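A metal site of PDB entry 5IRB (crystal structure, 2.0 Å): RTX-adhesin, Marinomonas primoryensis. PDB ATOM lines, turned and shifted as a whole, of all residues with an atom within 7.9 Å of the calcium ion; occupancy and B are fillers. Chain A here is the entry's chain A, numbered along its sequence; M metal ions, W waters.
OD1 of Asp 296 lies within hydrogen-bond range of N of Asn 300.
The side-chain carboxylate (OD1) of Asp 296 lies close to the backbone NH (N) of Ala 298 (3.2 Å).
The side-chain carboxylate (OD1) of Asp 296 sits at hydrogen-bond distance from the backbone NH (N) of Gly 299 (3.1 Å).
The backbone NH (N) of Ser 211 lies close to the side-chain amide nitrogen (ND2) of Asn 300.
The backbone carbonyl oxygen of Asp 209 is in hydrogen-bond range of the side-chain amide nitrogen of Asn 300 (2.8 Å).
Three residues have an atom within 4 Å of the calcium ion: Asp 209, Ser 211 and Asp 296.
The nearest printed residue that does not touch the calcium ion is Ala 212 (4.2 Å).
The calcium ion is bound by water W1 (2.1 Å).
The calcium ion is bound by OD2 of Asp 296 (2.2 Å).
Water W2 binds the calcium ion, at 2.3 Å.
The calcium ion is bound by O of Ser 211 (2.4 Å).
The side-chain carboxylate (OD1) of Asp 209 is bound to the calcium ion, at 2.4 Å.
The calcium ion is bound by water W3 (2.5 Å).
OD2 of Asp 209 is bound to the calcium ion (2.5 Å).
Water W3 bridges the side-chain carboxylate (OD2) of Asp 247 and the side-chain carboxylate (OD2) of Asp 213.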
ATOM      1  N   VAL A 124     -23.443 -17.838  -1.957  1.00  0.00           N
ATOM      2  CA  VAL A 124     -22.002 -17.588  -1.879  1.00  0.00           C
ATOM      3  C   VAL A 124     -21.396 -18.211  -0.611  1.00  0.00           C
ATOM      4  O   VAL A 124     -21.874 -18.003   0.517  1.00  0.00           O
ATOM      5  CB  VAL A 124     -21.708 -16.058  -1.915  1.00  0.00           C
ATOM      6  CG1 VAL A 124     -20.223 -15.791  -1.793  1.00  0.00           C
ATOM      7  CG2 VAL A 124     -22.266 -15.467  -3.192  1.00  0.00           C
ATOM      8  N   VAL A 208     -17.585 -18.868  -4.668  1.00  0.00           N
ATOM      9  CA  VAL A 208     -16.805 -18.900  -3.451  1.00  0.00           C
ATOM     10  C   VAL A 208     -16.075 -17.558  -3.308  1.00  0.00           C
ATOM     11  O   VAL A 208     -15.374 -17.124  -4.212  1.00  0.00           O
ATOM     12  CB  VAL A 208     -15.816 -20.086  -3.453  1.00  0.00           C
ATOM     13  CG1 VAL A 208     -14.938 -20.055  -2.214  1.00  0.00           C
ATOM     14  CG2 VAL A 208     -16.595 -21.426  -3.541  1.00  0.00           C
ATOM     15  N   ASP A 209     -16.286 -16.901  -2.170  1.00  0.00           N
ATOM     16  CA  ASP A 209     -15.668 -15.606  -1.863  1.00  0.00           C
ATOM     17  C   ASP A 209     -15.235 -15.609  -0.406  1.00  0.00           C
ATOM     18  O   ASP A 209     -16.061 -15.397   0.489  1.00  0.00           O
ATOM     19  CB  ASP A 209     -16.630 -14.449  -2.105  1.00  0.00           C
ATOM     20  CG  ASP A 209     -15.948 -13.078  -1.982  1.00  0.00           C
ATOM     21  OD1 ASP A 209     -14.846 -13.016  -1.380  1.00  0.00           O
ATOM     22  OD2 ASP A 209     -16.526 -12.066  -2.465  1.00  0.00           O
ATOM     23  N   THR A 210     -13.954 -15.856  -0.143  1.00  0.00           N
ATOM     24  CA  THR A 210     -13.514 -15.990   1.237  1.00  0.00           C
ATOM     25  C   THR A 210     -12.609 -14.848   1.709  1.00  0.00           C
ATOM     26  O   THR A 210     -11.927 -14.988   2.716  1.00  0.00           O
ATOM     27  CB  THR A 210     -12.772 -17.301   1.453  1.00  0.00           C
ATOM     28  OG1 THR A 210     -11.593 -17.306   0.635  1.00  0.00           O
ATOM     29  CG2 THR A 210     -13.658 -18.508   1.114  1.00  0.00           C
ATOM     30  N   SER A 211     -12.575 -13.730   1.012  1.00  0.00           N
ATOM     31  CA  SER A 211     -11.886 -12.579   1.596  1.00  0.00           C
ATOM     32  C   SER A 211     -12.420 -11.261   1.106  1.00  0.00           C
ATOM     33  O   SER A 211     -12.861 -11.136  -0.046  1.00  0.00           O
ATOM     34  CB  SER A 211     -10.370 -12.634   1.355  1.00  0.00           C
ATOM     35  OG  SER A 211     -10.059 -12.502  -0.011  1.00  0.00           O
ATOM     36  N   ALA A 212     -12.372 -10.299   2.006  1.00  0.00           N
ATOM     37  CA  ALA A 212     -12.653  -8.903   1.713  1.00  0.00           C
ATOM     38  C   ALA A 212     -11.319  -8.178   1.528  1.00  0.00           C
ATOM     39  O   ALA A 212     -10.291  -8.669   1.961  1.00  0.00           O
ATOM     40  CB  ALA A 212     -13.473  -8.266   2.838  1.00  0.00           C
ATOM     41  N   ASP A 213     -11.359  -7.039   0.847  1.00  0.00           N
ATOM     42  CA  ASP A 213     -10.144  -6.377   0.375  1.00  0.00           C
ATOM     43  C   ASP A 213      -9.868  -5.049   1.103  1.00  0.00           C
ATOM     44  O   ASP A 213     -10.723  -4.175   1.162  1.00  0.00           O
ATOM     45  CB  ASP A 213     -10.240  -6.107  -1.130  1.00  0.00           C
ATOM     46  CG  ASP A 213     -10.315  -7.399  -1.926  1.00  0.00           C
ATOM     47  OD1 ASP A 213      -9.553  -8.341  -1.599  1.00  0.00           O
ATOM     48  OD2 ASP A 213     -11.159  -7.487  -2.842  1.00  0.00           O
ATOM     49  N   ASP A 247     -12.729  -2.662  -0.176  1.00  0.00           N
ATOM     50  CA  ASP A 247     -14.120  -2.712   0.274  1.00  0.00           C
ATOM     51  C   ASP A 247     -14.485  -1.637   1.282  1.00  0.00           C
ATOM     52  O   ASP A 247     -15.561  -1.699   1.881  1.00  0.00           O
ATOM     53  CB  ASP A 247     -14.398  -4.094   0.872  1.00  0.00           C
ATOM     54  CG  ASP A 247     -14.499  -5.156  -0.174  1.00  0.00           C
ATOM     55  OD1 ASP A 247     -15.097  -4.887  -1.238  1.00  0.00           O
ATOM     56  OD2 ASP A 247     -13.906  -6.218   0.042  1.00  0.00           O
ATOM     57  N   SER A 295     -16.358  -4.633   5.121  1.00  0.00           N
ATOM     58  CA  SER A 295     -16.887  -5.925   4.740  1.00  0.00           C
ATOM     59  C   SER A 295     -17.356  -5.885   3.289  1.00  0.00           C
ATOM     60  O   SER A 295     -17.674  -4.826   2.769  1.00  0.00           O
ATOM     61  CB  SER A 295     -18.003  -6.323   5.721  1.00  0.00           C
ATOM     62  OG  SER A 295     -19.073  -5.418   5.563  1.00  0.00           O
ATOM     63  N   ASP A 296     -17.307  -7.044   2.624  1.00  0.00           N
ATOM     64  CA  ASP A 296     -17.888  -7.186   1.287  1.00  0.00           C
ATOM     65  C   ASP A 296     -19.316  -7.745   1.349  1.00  0.00           C
ATOM     66  O   ASP A 296     -19.830  -8.037   2.440  1.00  0.00           O
ATOM     67  CB  ASP A 296     -16.947  -8.015   0.374  1.00  0.00           C
ATOM     68  CG  ASP A 296     -16.826  -9.501   0.796  1.00  0.00           C
ATOM     69  OD1 ASP A 296     -17.579  -9.947   1.693  1.00  0.00           O
ATOM     70  OD2 ASP A 296     -15.974 -10.209   0.206  1.00  0.00           O
ATOM     71  N   ALA A 297     -19.971  -7.869   0.205  1.00  0.00           N
ATOM     72  CA  ALA A 297     -21.369  -8.314   0.186  1.00  0.00           C
ATOM     73  C   ALA A 297     -21.513  -9.743   0.688  1.00  0.00           C
ATOM     74  O   ALA A 297     -22.543 -10.087   1.263  1.00  0.00           O
ATOM     75  CB  ALA A 297     -21.977  -8.197  -1.238  1.00  0.00           C
ATOM     76  N   ALA A 298     -20.486 -10.571   0.487  1.00  0.00           N
ATOM     77  CA  ALA A 298     -20.496 -11.934   1.036  1.00  0.00           C
ATOM     78  C   ALA A 298     -20.439 -11.996   2.544  1.00  0.00           C
ATOM     79  O   ALA A 298     -20.727 -13.040   3.120  1.00  0.00           O
ATOM     80  CB  ALA A 298     -19.351 -12.744   0.467  1.00  0.00           C
ATOM     81  N   GLY A 299     -20.066 -10.890   3.198  1.00  0.00           N
ATOM     82  CA  GLY A 299     -20.021 -10.857   4.648  1.00  0.00           C
ATOM     83  C   GLY A 299     -18.653 -11.065   5.253  1.00  0.00           C
ATOM     84  O   GLY A 299     -18.525 -11.136   6.480  1.00  0.00           O
ATOM     85  N   ASN A 300     -17.618 -11.169   4.424  1.00  0.00           N
ATOM     86  CA  ASN A 300     -16.269 -11.248   4.931  1.00  0.00           C
ATOM     87  C   ASN A 300     -15.891  -9.898   5.510  1.00  0.00           C
ATOM     88  O   ASN A 300     -16.440  -8.896   5.099  1.00  0.00           O
ATOM     89  CB  ASN A 300     -15.287 -11.621   3.826  1.00  0.00           C
ATOM     90  CG  ASN A 300     -15.625 -12.937   3.182  1.00  0.00           C
ATOM     91  OD1 ASN A 300     -15.741 -13.952   3.865  1.00  0.00           O
ATOM     92  ND2 ASN A 300     -15.770 -12.923   1.865  1.00  0.00           N
HETATM   93 CA    CA M   1     -14.658 -10.624  -1.517  1.00  0.00          CA
HETATM   94  O   HOH W   1     -13.247 -11.087  -3.026  1.00  0.00           O
HETATM   95  O   HOH W   2     -16.085  -9.411  -2.924  1.00  0.00           O
HETATM   96  O   HOH W   3     -13.694  -8.289  -1.379  1.00  0.00           O
